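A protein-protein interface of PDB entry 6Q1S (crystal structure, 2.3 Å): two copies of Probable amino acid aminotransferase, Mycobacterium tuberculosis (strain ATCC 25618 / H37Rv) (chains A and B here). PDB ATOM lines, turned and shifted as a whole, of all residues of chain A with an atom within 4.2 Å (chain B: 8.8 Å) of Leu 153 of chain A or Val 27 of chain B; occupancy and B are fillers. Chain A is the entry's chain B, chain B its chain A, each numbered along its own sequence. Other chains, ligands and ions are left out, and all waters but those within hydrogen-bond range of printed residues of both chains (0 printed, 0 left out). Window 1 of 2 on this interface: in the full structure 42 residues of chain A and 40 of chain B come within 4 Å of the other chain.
Hydrophobic or aromatic side chains of chain A within 4 Å of the printed part of chain B: Met 110, Leu 153 and Tyr 155. Printed residues of chain B that touch a printed residue of chain A: Ala 21, Ala 25, Ala 26, Val 27, Arg 28, Gly 29, Glu 100, Leu 153, Ser 154, Tyr 155 and Ala 156. Hydrophobic or aromatic side chains of chain B within 4 Å of the printed part of chain A: Val 27 and Ala 156. Along chain B the printed residues that touch a printed residue of chain A span positions 21 to 156.
Among the printed residues, merely in contact across the chains: Leu 153 of chain A with Ala 26 of chain B (3.3 Å), Ser 154 of chain A with Ser 154 of chain B (3.4 Å), Ser 154 of chain A with Tyr 155 of chain B (3.6 Å), Tyr 155 of chain A with Ser 154 of chain B (3.6 Å), Gly 29 of chain A with Ala 156 of chain B (3.6 Å), Leu 153 of chain A with Val 27 of chain B (3.6 Å), Met 110 of chain A with Val 27 of chain B (3.7 Å), Ala 25 of chain A with Ala 26 of chain B (3.7 Å), Thr 152 of chain A with Ala 156 of chain B (3.9 Å) and Ser 154 of chain A with Arg 28 of chain B (3.97 Å).
Of the printed residues of chain B, Ala 25 of chain A touches Ala 25 and Ala 26. No residue of chain B comes within 4 Å of Gly 31 of chain A. Printed residues of chain B within 4 Å of Arg 92 of chain A: Glu 100. Of the printed residues of chain B, Met 110 of chain A touches Ala 21 and Val 27. Of chain B, only Ala 26, Val 27, Arg 28 and Gly 29 come within 4 Å of Leu 153 of chain A. Ser 154 of chain A touches just these residues of chain B: Arg 28 (3.97 Å), Ser 154 (3.4 Å), Tyr 155 (3.6 Å) and Ala 156 (3.1 Å). Printed residues of chain B within 4 Å of Tyr 155 of chain A: Arg 28 and Ser 154. His 20 of chain B touches none of the printed residues of chain A. Printed residues of chain A within 4 Å of Ala 26 of chain B: Ala 25 (3.7 Å) and Leu 153 (3.3 Å). Printed residues of chain A within 4 Å of Val 27 of chain B: Met 110 and Leu 153. The nearest residue of chain B that does not touch Leu 153 of chain A is Ser 154 of chain B (4.7 Å). The nearest printed residue of chain B that does not touch Ala 25 of chain A is Gly 29 of chain B (4.8 Å).
The backbone carbonyl oxygen of Leu 153 of chain A lies close to the backbone carbonyl oxygen of Arg 28 of chain B, at 3.2 Å. The backbone NH (N) of Gly 29 of chain B lies within hydrogen-bond range of the backbone carbonyl oxygen (O) of Leu 153 of chain A (2.8 Å). The backbone carbonyl oxygen (O) of Arg 28 of chain B sits at hydrogen-bond distance from the backbone NH (N) of Tyr 155 of chain A. The backbone carbonyl oxygen (O) of Ala 25 of chain A sits close to the backbone carbonyl oxygen (O) of Ala 25 of chain B, 2.9 Å away. The backbone carbonyl oxygen (O) of Ala 21 of chain B sits close to the side-chain sulfur (SD) of Met 110 of chain A (3.7 Å). The backbone NH (N) of Gly 29 of chain A lies within hydrogen-bond range of the backbone carbonyl oxygen (O) of Leu 153 of chain B (3.0 Å). The side-chain carboxylate (OE2) of Glu 100 of chain B is in salt-bridge range of the guanidinium group (NH1) of Arg 92 of chain A (2.5 Å). N of Ala 156 of chain B lies close to OG of Ser 154 of chain A, 3.2 Å away.
The backbone NH of Arg 92 of chain A sits at hydrogen-bond distance from the backbone carbonyl oxygen of Met 110 of chain A. The guanidinium group of Arg 28 of chain B lies within salt-bridge range of the side-chain carboxylate of Glu 100 of chain B. The backbone carbonyl oxygen (O) of Gly 29 of chain A sits at hydrogen-bond distance from the side-chain hydroxyl (OG) of Ser 154 of chain A (2.7 Å). The side-chain hydroxyl (OG1) of Thr 152 of chain A lies close to the backbone NH (N) of Ser 154 of chain A (3.2 Å). O of Leu 24 of chain B is in hydrogen-bond range of N of Gly 29 of chain B, at 3.2 Å. N of Leu 153 of chain B sits at hydrogen-bond distance from O of Gly 31 of chain B, 2.8 Å away.
Ala 25 of chain A touches its own counterpart, Ala 25 of chain B. Gly 29 of chain A touches Leu 153 of chain B, and with the chains exchanged Leu 153 of chain A touches Gly 29 of chain B. Ser 154 of chain B touches its own counterpart, Ser 154 of chain A. Ser 154 of chain A touches Tyr 155 of chain B, and with the chains exchanged Tyr 155 of chain A touches Ser 154 of chain B. Positions printed for both chains: 25, 29, 31, 153, 154 and 155. Of the 18 pairs that touch across the chains among the printed residues, 6 have their exchanged pair printed and touching as well.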
ATOM      1  N   ALA A  25      -3.206 -18.489  13.977  1.00  0.00           N
ATOM      2  CA  ALA A  25      -2.230 -17.818  13.126  1.00  0.00           C
ATOM      3  C   ALA A  25      -2.867 -16.695  12.326  1.00  0.00           C
ATOM      4  O   ALA A  25      -2.218 -15.677  12.061  1.00  0.00           O
ATOM      5  CB  ALA A  25      -1.571 -18.821  12.182  1.00  0.00           C
ATOM      6  N   GLY A  29      -2.264 -13.897  14.718  1.00  0.00           N
ATOM      7  CA  GLY A  29      -0.845 -14.065  14.445  1.00  0.00           C
ATOM      8  C   GLY A  29      -0.104 -14.852  15.501  1.00  0.00           C
ATOM      9  O   GLY A  29       1.082 -14.596  15.742  1.00  0.00           O
ATOM     10  N   GLY A  31       1.763 -17.596  16.593  1.00  0.00           N
ATOM     11  CA  GLY A  31       2.569 -18.731  16.183  1.00  0.00           C
ATOM     12  C   GLY A  31       3.978 -18.280  15.877  1.00  0.00           C
ATOM     13  O   GLY A  31       4.300 -17.091  15.934  1.00  0.00           O
ATOM     14  N   VAL A  32       4.822 -19.258  15.551  1.00  0.00           N
ATOM     15  CA  VAL A  32       6.210 -19.000  15.199  1.00  0.00           C
ATOM     16  C   VAL A  32       6.483 -19.612  13.832  1.00  0.00           C
ATOM     17  O   VAL A  32       5.767 -20.505  13.370  1.00  0.00           O
ATOM     18  CB  VAL A  32       7.191 -19.557  16.251  1.00  0.00           C
ATOM     19  CG1 VAL A  32       6.902 -18.952  17.615  1.00  0.00           C
ATOM     20  CG2 VAL A  32       7.112 -21.076  16.306  1.00  0.00           C
ATOM     21  N   PHE A  33       7.536 -19.123  13.180  1.00  0.00           N
ATOM     22  CA  PHE A  33       7.889 -19.641  11.868  1.00  0.00           C
ATOM     23  C   PHE A  33       9.385 -19.496  11.636  1.00  0.00           C
ATOM     24  O   PHE A  33      10.101 -18.846  12.401  1.00  0.00           O
ATOM     25  CB  PHE A  33       7.096 -18.945  10.753  1.00  0.00           C
ATOM     26  CG  PHE A  33       7.661 -17.618  10.330  1.00  0.00           C
ATOM     27  CD1 PHE A  33       7.441 -16.480  11.086  1.00  0.00           C
ATOM     28  CD2 PHE A  33       8.387 -17.507   9.156  1.00  0.00           C
ATOM     29  CE1 PHE A  33       7.954 -15.256  10.689  1.00  0.00           C
ATOM     30  CE2 PHE A  33       8.903 -16.288   8.752  1.00  0.00           C
ATOM     31  CZ  PHE A  33       8.684 -15.161   9.520  1.00  0.00           C
ATOM     32  N   ARG A  92       9.504 -22.378   4.104  1.00  0.00           N
ATOM     33  CA  ARG A  92       9.069 -21.788   5.361  1.00  0.00           C
ATOM     34  C   ARG A  92       8.361 -22.834   6.209  1.00  0.00           C
ATOM     35  O   ARG A  92       7.601 -23.654   5.689  1.00  0.00           O
ATOM     36  CB  ARG A  92       8.131 -20.593   5.128  1.00  0.00           C
ATOM     37  CG  ARG A  92       8.858 -19.278   4.885  1.00  0.00           C
ATOM     38  CD  ARG A  92       7.907 -18.186   4.412  1.00  0.00           C
ATOM     39  NE  ARG A  92       7.183 -18.530   3.191  1.00  0.00           N
ATOM     40  CZ  ARG A  92       6.225 -17.773   2.663  1.00  0.00           C
ATOM     41  NH1 ARG A  92       5.886 -16.631   3.247  1.00  0.00           N
ATOM     42  NH2 ARG A  92       5.606 -18.156   1.555  1.00  0.00           N
ATOM     43  N   ILE A  94       5.701 -23.198   9.172  1.00  0.00           N
ATOM     44  CA  ILE A  94       4.640 -22.477   9.869  1.00  0.00           C
ATOM     45  C   ILE A  94       4.182 -23.322  11.049  1.00  0.00           C
ATOM     46  O   ILE A  94       3.757 -24.469  10.873  1.00  0.00           O
ATOM     47  CB  ILE A  94       3.466 -22.153   8.934  1.00  0.00           C
ATOM     48  CG1 ILE A  94       3.973 -21.494   7.651  1.00  0.00           C
ATOM     49  CG2 ILE A  94       2.459 -21.256   9.643  1.00  0.00           C
ATOM     50  CD1 ILE A  94       4.609 -20.139   7.870  1.00  0.00           C
ATOM     51  N   MET A 110       6.128 -25.126   3.811  1.00  0.00           N
ATOM     52  CA  MET A 110       5.719 -24.491   2.566  1.00  0.00           C
ATOM     53  C   MET A 110       6.935 -24.019   1.785  1.00  0.00           C
ATOM     54  O   MET A 110       7.821 -23.370   2.348  1.00  0.00           O
ATOM     55  CB  MET A 110       4.784 -23.311   2.846  1.00  0.00           C
ATOM     56  CG  MET A 110       4.393 -22.530   1.616  1.00  0.00           C
ATOM     57  SD  MET A 110       3.024 -21.408   1.940  1.00  0.00           S
ATOM     58  CE  MET A 110       3.572 -20.671   3.475  1.00  0.00           C
ATOM     59  N   THR A 152       7.992 -14.726  15.469  1.00  0.00           N
ATOM     60  CA  THR A 152       6.575 -15.046  15.442  1.00  0.00           C
ATOM     61  C   THR A 152       5.975 -14.722  14.079  1.00  0.00           C
ATOM     62  O   THR A 152       6.597 -14.084  13.228  1.00  0.00           O
ATOM     63  CB  THR A 152       5.820 -14.286  16.537  1.00  0.00           C
ATOM     64  OG1 THR A 152       5.669 -12.913  16.153  1.00  0.00           O
ATOM     65  CG2 THR A 152       6.579 -14.356  17.852  1.00  0.00           C
ATOM     66  N   LEU A 153       4.744 -15.184  13.880  1.00  0.00           N
ATOM     67  CA  LEU A 153       3.987 -14.899  12.669  1.00  0.00           C
ATOM     68  C   LEU A 153       3.366 -13.510  12.669  1.00  0.00           C
ATOM     69  O   LEU A 153       2.660 -13.169  11.717  1.00  0.00           O
ATOM     70  CB  LEU A 153       2.885 -15.943  12.482  1.00  0.00           C
ATOM     71  CG  LEU A 153       3.343 -17.375  12.215  1.00  0.00           C
ATOM     72  CD1 LEU A 153       2.193 -18.348  12.396  1.00  0.00           C
ATOM     73  CD2 LEU A 153       3.898 -17.466  10.809  1.00  0.00           C
ATOM     74  N   SER A 154       3.598 -12.708  13.708  1.00  0.00           N
ATOM     75  CA  SER A 154       2.985 -11.386  13.820  1.00  0.00           C
ATOM     76  C   SER A 154       3.952 -10.345  13.263  1.00  0.00           C
ATOM     77  O   SER A 154       4.608  -9.598  13.991  1.00  0.00           O
ATOM     78  CB  SER A 154       2.611 -11.104  15.268  1.00  0.00           C
ATOM     79  OG  SER A 154       1.513 -11.905  15.664  1.00  0.00           O
ATOM     80  N   TYR A 155       4.020 -10.287  11.933  1.00  0.00           N
ATOM     81  CA  TYR A 155       4.988  -9.449  11.236  1.00  0.00           C
ATOM     82  C   TYR A 155       4.350  -8.245  10.552  1.00  0.00           C
ATOM     83  O   TYR A 155       4.922  -7.706   9.600  1.00  0.00           O
ATOM     84  CB  TYR A 155       5.761 -10.278  10.212  1.00  0.00           C
ATOM     85  CG  TYR A 155       7.124 -10.710  10.690  1.00  0.00           C
ATOM     86  CD1 TYR A 155       7.283 -11.340  11.917  1.00  0.00           C
ATOM     87  CD2 TYR A 155       8.255 -10.475   9.924  1.00  0.00           C
ATOM     88  CE1 TYR A 155       8.529 -11.734  12.361  1.00  0.00           C
ATOM     89  CE2 TYR A 155       9.507 -10.862  10.359  1.00  0.00           C
ATOM     90  CZ  TYR A 155       9.638 -11.492  11.578  1.00  0.00           C
ATOM     91  OH  TYR A 155      10.883 -11.881  12.016  1.00  0.00           O
ATOM     92  N   LEU B  19      -8.930 -20.757   4.642  1.00  0.00           N
ATOM     93  CA  LEU B  19      -7.764 -20.010   4.201  1.00  0.00           C
ATOM     94  C   LEU B  19      -6.716 -20.943   3.611  1.00  0.00           C
ATOM     95  O   LEU B  19      -6.531 -22.069   4.082  1.00  0.00           O
ATOM     96  CB  LEU B  19      -7.164 -19.223   5.365  1.00  0.00           C
ATOM     97  CG  LEU B  19      -8.207 -18.461   6.181  1.00  0.00           C
ATOM     98  CD1 LEU B  19      -7.653 -18.078   7.537  1.00  0.00           C
ATOM     99  CD2 LEU B  19      -8.669 -17.231   5.418  1.00  0.00           C
ATOM    100  N   HIS B  20      -6.042 -20.469   2.569  1.00  0.00           N
ATOM    101  CA  HIS B  20      -4.934 -21.201   1.985  1.00  0.00           C
ATOM    102  C   HIS B  20      -3.690 -21.039   2.853  1.00  0.00           C
ATOM    103  O   HIS B  20      -3.612 -20.170   3.726  1.00  0.00           O
ATOM    104  CB  HIS B  20      -4.652 -20.719   0.562  1.00  0.00           C
ATOM    105  CG  HIS B  20      -5.772 -20.975  -0.399  1.00  0.00           C
ATOM    106  ND1 HIS B  20      -6.926 -20.222  -0.417  1.00  0.00           N
ATOM    107  CD2 HIS B  20      -5.907 -21.893  -1.386  1.00  0.00           C
ATOM    108  CE1 HIS B  20      -7.728 -20.670  -1.368  1.00  0.00           C
ATOM    109  NE2 HIS B  20      -7.132 -21.683  -1.971  1.00  0.00           N
ATOM    110  N   ALA B  21      -2.696 -21.888   2.595  1.00  0.00           N
ATOM    111  CA  ALA B  21      -1.485 -21.881   3.406  1.00  0.00           C
ATOM    112  C   ALA B  21      -0.647 -20.625   3.201  1.00  0.00           C
ATOM    113  O   ALA B  21       0.221 -20.336   4.031  1.00  0.00           O
ATOM    114  CB  ALA B  21      -0.644 -23.117   3.102  1.00  0.00           C
ATOM    115  N   ASP B  22      -0.886 -19.874   2.128  1.00  0.00           N
ATOM    116  CA  ASP B  22      -0.091 -18.694   1.812  1.00  0.00           C
ATOM    117  C   ASP B  22      -0.832 -17.389   2.078  1.00  0.00           C
ATOM    118  O   ASP B  22      -0.391 -16.334   1.612  1.00  0.00           O
ATOM    119  CB  ASP B  22       0.369 -18.748   0.354  1.00  0.00           C
ATOM    120  CG  ASP B  22      -0.776 -18.993  -0.609  1.00  0.00           C
ATOM    121  OD1 ASP B  22      -1.923 -19.151  -0.143  1.00  0.00           O
ATOM    122  OD2 ASP B  22      -0.529 -19.033  -1.832  1.00  0.00           O
ATOM    123  N   ASP B  23      -1.940 -17.430   2.813  1.00  0.00           N
ATOM    124  CA  ASP B  23      -2.651 -16.204   3.153  1.00  0.00           C
ATOM    125  C   ASP B  23      -1.804 -15.346   4.084  1.00  0.00           C
ATOM    126  O   ASP B  23      -1.262 -15.839   5.077  1.00  0.00           O
ATOM    127  CB  ASP B  23      -3.997 -16.532   3.796  1.00  0.00           C
ATOM    128  CG  ASP B  23      -4.927 -15.334   3.842  1.00  0.00           C
ATOM    129  OD1 ASP B  23      -4.657 -14.398   4.626  1.00  0.00           O
ATOM    130  OD2 ASP B  23      -5.920 -15.321   3.086  1.00  0.00           O
ATOM    131  N   LEU B  24      -1.701 -14.053   3.763  1.00  0.00           N
ATOM    132  CA  LEU B  24      -0.829 -13.155   4.513  1.00  0.00           C
ATOM    133  C   LEU B  24      -1.285 -12.949   5.951  1.00  0.00           C
ATOM    134  O   LEU B  24      -0.502 -12.448   6.766  1.00  0.00           O
ATOM    135  CB  LEU B  24      -0.718 -11.806   3.804  1.00  0.00           C
ATOM    136  CG  LEU B  24       0.172 -11.802   2.561  1.00  0.00           C
ATOM    137  CD1 LEU B  24      -0.189 -10.658   1.635  1.00  0.00           C
ATOM    138  CD2 LEU B  24       1.631 -11.722   2.971  1.00  0.00           C
ATOM    139  N   ALA B  25      -2.531 -13.292   6.280  1.00  0.00           N
ATOM    140  CA  ALA B  25      -2.945 -13.265   7.677  1.00  0.00           C
ATOM    141  C   ALA B  25      -2.214 -14.320   8.496  1.00  0.00           C
ATOM    142  O   ALA B  25      -1.910 -14.091   9.671  1.00  0.00           O
ATOM    143  CB  ALA B  25      -4.455 -13.466   7.790  1.00  0.00           C
ATOM    144  N   ALA B  26      -1.915 -15.470   7.893  1.00  0.00           N
ATOM    145  CA  ALA B  26      -1.301 -16.577   8.611  1.00  0.00           C
ATOM    146  C   ALA B  26       0.221 -16.555   8.546  1.00  0.00           C
ATOM    147  O   ALA B  26       0.886 -16.876   9.538  1.00  0.00           O
ATOM    148  CB  ALA B  26      -1.817 -17.908   8.060  1.00  0.00           C
ATOM    149  N   VAL B  27       0.791 -16.177   7.404  1.00  0.00           N
ATOM    150  CA  VAL B  27       2.238 -16.235   7.240  1.00  0.00           C
ATOM    151  C   VAL B  27       2.930 -14.986   7.780  1.00  0.00           C
ATOM    152  O   VAL B  27       4.113 -15.044   8.138  1.00  0.00           O
ATOM    153  CB  VAL B  27       2.597 -16.472   5.764  1.00  0.00           C
ATOM    154  CG1 VAL B  27       2.147 -17.858   5.330  1.00  0.00           C
ATOM    155  CG2 VAL B  27       1.977 -15.403   4.882  1.00  0.00           C
ATOM    156  N   ARG B  28       2.230 -13.847   7.836  1.00  0.00           N
ATOM    157  CA  ARG B  28       2.842 -12.606   8.296  1.00  0.00           C
ATOM    158  C   ARG B  28       1.965 -11.830   9.273  1.00  0.00           C
ATOM    159  O   ARG B  28       2.337 -10.711   9.651  1.00  0.00           O
ATOM    160  CB  ARG B  28       3.208 -11.696   7.111  1.00  0.00           C
ATOM    161  CG  ARG B  28       4.191 -12.298   6.119  1.00  0.00           C
ATOM    162  CD  ARG B  28       4.910 -11.211   5.331  1.00  0.00           C
ATOM    163  NE  ARG B  28       5.979 -11.753   4.494  1.00  0.00           N
ATOM    164  CZ  ARG B  28       5.993 -11.701   3.167  1.00  0.00           C
ATOM    165  NH1 ARG B  28       7.008 -12.221   2.492  1.00  0.00           N
ATOM    166  NH2 ARG B  28       4.998 -11.118   2.511  1.00  0.00           N
ATOM    167  N   GLY B  29       0.829 -12.378   9.700  1.00  0.00           N
ATOM    168  CA  GLY B  29      -0.086 -11.625  10.541  1.00  0.00           C
ATOM    169  C   GLY B  29      -0.514 -10.317   9.917  1.00  0.00           C
ATOM    170  O   GLY B  29      -0.791  -9.349  10.633  1.00  0.00           O
ATOM    171  N   ASP B  30      -0.579 -10.271   8.587  1.00  0.00           N
ATOM    172  CA  ASP B  30      -0.717  -9.032   7.826  1.00  0.00           C
ATOM    173  C   ASP B  30      -2.189  -8.766   7.533  1.00  0.00           C
ATOM    174  O   ASP B  30      -2.727  -9.188   6.507  1.00  0.00           O
ATOM    175  CB  ASP B  30       0.096  -9.119   6.543  1.00  0.00           C
ATOM    176  CG  ASP B  30       0.323  -7.771   5.905  1.00  0.00           C
ATOM    177  OD1 ASP B  30      -0.031  -6.751   6.531  1.00  0.00           O
ATOM    178  OD2 ASP B  30       0.840  -7.734   4.769  1.00  0.00           O
ATOM    179  N   GLY B  31      -2.842  -8.046   8.435  1.00  0.00           N
ATOM    180  CA  GLY B  31      -4.238  -7.694   8.239  1.00  0.00           C
ATOM    181  C   GLY B  31      -4.747  -6.914   9.428  1.00  0.00           C
ATOM    182  O   GLY B  31      -4.032  -6.698  10.412  1.00  0.00           O
ATOM    183  N   SER B  96      -7.650  -9.289   5.739  1.00  0.00           N
ATOM    184  CA  SER B  96      -6.227  -9.474   5.504  1.00  0.00           C
ATOM    185  C   SER B  96      -5.866  -9.033   4.091  1.00  0.00           C
ATOM    186  O   SER B  96      -6.728  -8.843   3.229  1.00  0.00           O
ATOM    187  CB  SER B  96      -5.820 -10.936   5.733  1.00  0.00           C
ATOM    188  OG  SER B  96      -5.752 -11.655   4.515  1.00  0.00           O
ATOM    189  N   GLY B  98      -4.697 -10.673   1.801  1.00  0.00           N
ATOM    190  CA  GLY B  98      -4.938 -11.707   0.817  1.00  0.00           C
ATOM    191  C   GLY B  98      -3.794 -12.696   0.762  1.00  0.00           C
ATOM    192  O   GLY B  98      -2.900 -12.723   1.612  1.00  0.00           O
ATOM    193  N   ARG B  99      -3.825 -13.521  -0.276  1.00  0.00           N
ATOM    194  CA  ARG B  99      -2.805 -14.544  -0.422  1.00  0.00           C
ATOM    195  C   ARG B  99      -1.473 -13.916  -0.811  1.00  0.00           C
ATOM    196  O   ARG B  99      -1.418 -12.837  -1.407  1.00  0.00           O
ATOM    197  CB  ARG B  99      -3.226 -15.573  -1.469  1.00  0.00           C
ATOM    198  CG  ARG B  99      -4.349 -16.486  -1.020  1.00  0.00           C
ATOM    199  CD  ARG B  99      -4.706 -17.477  -2.111  1.00  0.00           C
ATOM    200  NE  ARG B  99      -3.638 -18.445  -2.345  1.00  0.00           N
ATOM    201  CZ  ARG B  99      -3.701 -19.418  -3.249  1.00  0.00           C
ATOM    202  NH1 ARG B  99      -4.783 -19.550  -4.004  1.00  0.00           N
ATOM    203  NH2 ARG B  99      -2.686 -20.258  -3.399  1.00  0.00           N
ATOM    204  N   GLU B 100      -0.392 -14.601  -0.455  1.00  0.00           N
ATOM    205  CA  GLU B 100       0.935 -14.142  -0.836  1.00  0.00           C
ATOM    206  C   GLU B 100       1.073 -14.211  -2.349  1.00  0.00           C
ATOM    207  O   GLU B 100       0.833 -15.259  -2.957  1.00  0.00           O
ATOM    208  CB  GLU B 100       2.005 -14.993  -0.157  1.00  0.00           C
ATOM    209  CG  GLU B 100       3.404 -14.412  -0.224  1.00  0.00           C
ATOM    210  CD  GLU B 100       4.436 -15.330   0.395  1.00  0.00           C
ATOM    211  OE1 GLU B 100       5.033 -16.138  -0.347  1.00  0.00           O
ATOM    212  OE2 GLU B 100       4.641 -15.253   1.624  1.00  0.00           O
ATOM    213  N   GLY B 101       1.448 -13.089  -2.961  1.00  0.00           N
ATOM    214  CA  GLY B 101       1.532 -12.995  -4.400  1.00  0.00           C
ATOM    215  C   GLY B 101       0.217 -12.733  -5.098  1.00  0.00           C
ATOM    216  O   GLY B 101       0.224 -12.327  -6.267  1.00  0.00           O
ATOM    217  N   LEU B 153      -3.973  -7.812  12.967  1.00  0.00           N
ATOM    218  CA  LEU B 153      -4.055  -9.219  13.331  1.00  0.00           C
ATOM    219  C   LEU B 153      -2.787  -9.731  13.991  1.00  0.00           C
ATOM    220  O   LEU B 153      -2.710 -10.922  14.298  1.00  0.00           O
ATOM    221  CB  LEU B 153      -4.347 -10.073  12.095  1.00  0.00           C
ATOM    222  CG  LEU B 153      -5.685  -9.903  11.379  1.00  0.00           C
ATOM    223  CD1 LEU B 153      -5.639 -10.572  10.016  1.00  0.00           C
ATOM    224  CD2 LEU B 153      -6.795 -10.495  12.222  1.00  0.00           C
ATOM    225  N   SER B 154      -1.788  -8.873  14.197  1.00  0.00           N
ATOM    226  CA  SER B 154      -0.501  -9.293  14.748  1.00  0.00           C
ATOM    227  C   SER B 154      -0.512  -9.071  16.258  1.00  0.00           C
ATOM    228  O   SER B 154       0.091  -8.138  16.792  1.00  0.00           O
ATOM    229  CB  SER B 154       0.631  -8.548  14.057  1.00  0.00           C
ATOM    230  OG  SER B 154       0.775  -9.015  12.726  1.00  0.00           O
ATOM    231  N   TYR B 155      -1.187  -9.985  16.957  1.00  0.00           N
ATOM    232  CA  TYR B 155      -1.435  -9.883  18.390  1.00  0.00           C
ATOM    233  C   TYR B 155      -0.610 -10.883  19.197  1.00  0.00           C
ATOM    234  O   TYR B 155      -0.997 -11.258  20.305  1.00  0.00           O
ATOM    235  CB  TYR B 155      -2.922 -10.073  18.678  1.00  0.00           C
ATOM    236  CG  TYR B 155      -3.676  -8.784  18.892  1.00  0.00           C
ATOM    237  CD1 TYR B 155      -3.562  -7.731  17.991  1.00  0.00           C
ATOM    238  CD2 TYR B 155      -4.518  -8.624  19.984  1.00  0.00           C
ATOM    239  CE1 TYR B 155      -4.252  -6.548  18.181  1.00  0.00           C
ATOM    240  CE2 TYR B 155      -5.215  -7.446  20.181  1.00  0.00           C
ATOM    241  CZ  TYR B 155      -5.079  -6.414  19.276  1.00  0.00           C
ATOM    242  OH  TYR B 155      -5.770  -5.238  19.468  1.00  0.00           O
ATOM    243  N   ALA B 156       0.531 -11.322  18.657  1.00  0.00           N
ATOM    244  CA  ALA B 156       1.344 -12.304  19.369  1.00  0.00           C
ATOM    245  C   ALA B 156       1.871 -11.736  20.679  1.00  0.00           C
ATOM    246  O   ALA B 156       1.903 -12.435  21.698  1.00  0.00           O
ATOM    247  CB  ALA B 156       2.502 -12.777  18.491  1.00  0.00           C
ATOM    248  N   VAL B 157       2.298 -10.472  20.672  1.00  0.00           N
ATOM    249  CA  VAL B 157       2.802  -9.862  21.897  1.00  0.00           C
ATOM    250  C   VAL B 157       1.663  -9.633  22.884  1.00  0.00           C
ATOM    251  O   VAL B 157       1.818  -9.847  24.091  1.00  0.00           O
ATOM    252  CB  VAL B 157       3.552  -8.556  21.573  1.00  0.00           C
ATOM    253  CG1 VAL B 157       3.914  -7.815  22.849  1.00  0.00           C
ATOM    254  CG2 VAL B 157       4.801  -8.856  20.762  1.00  0.00           C
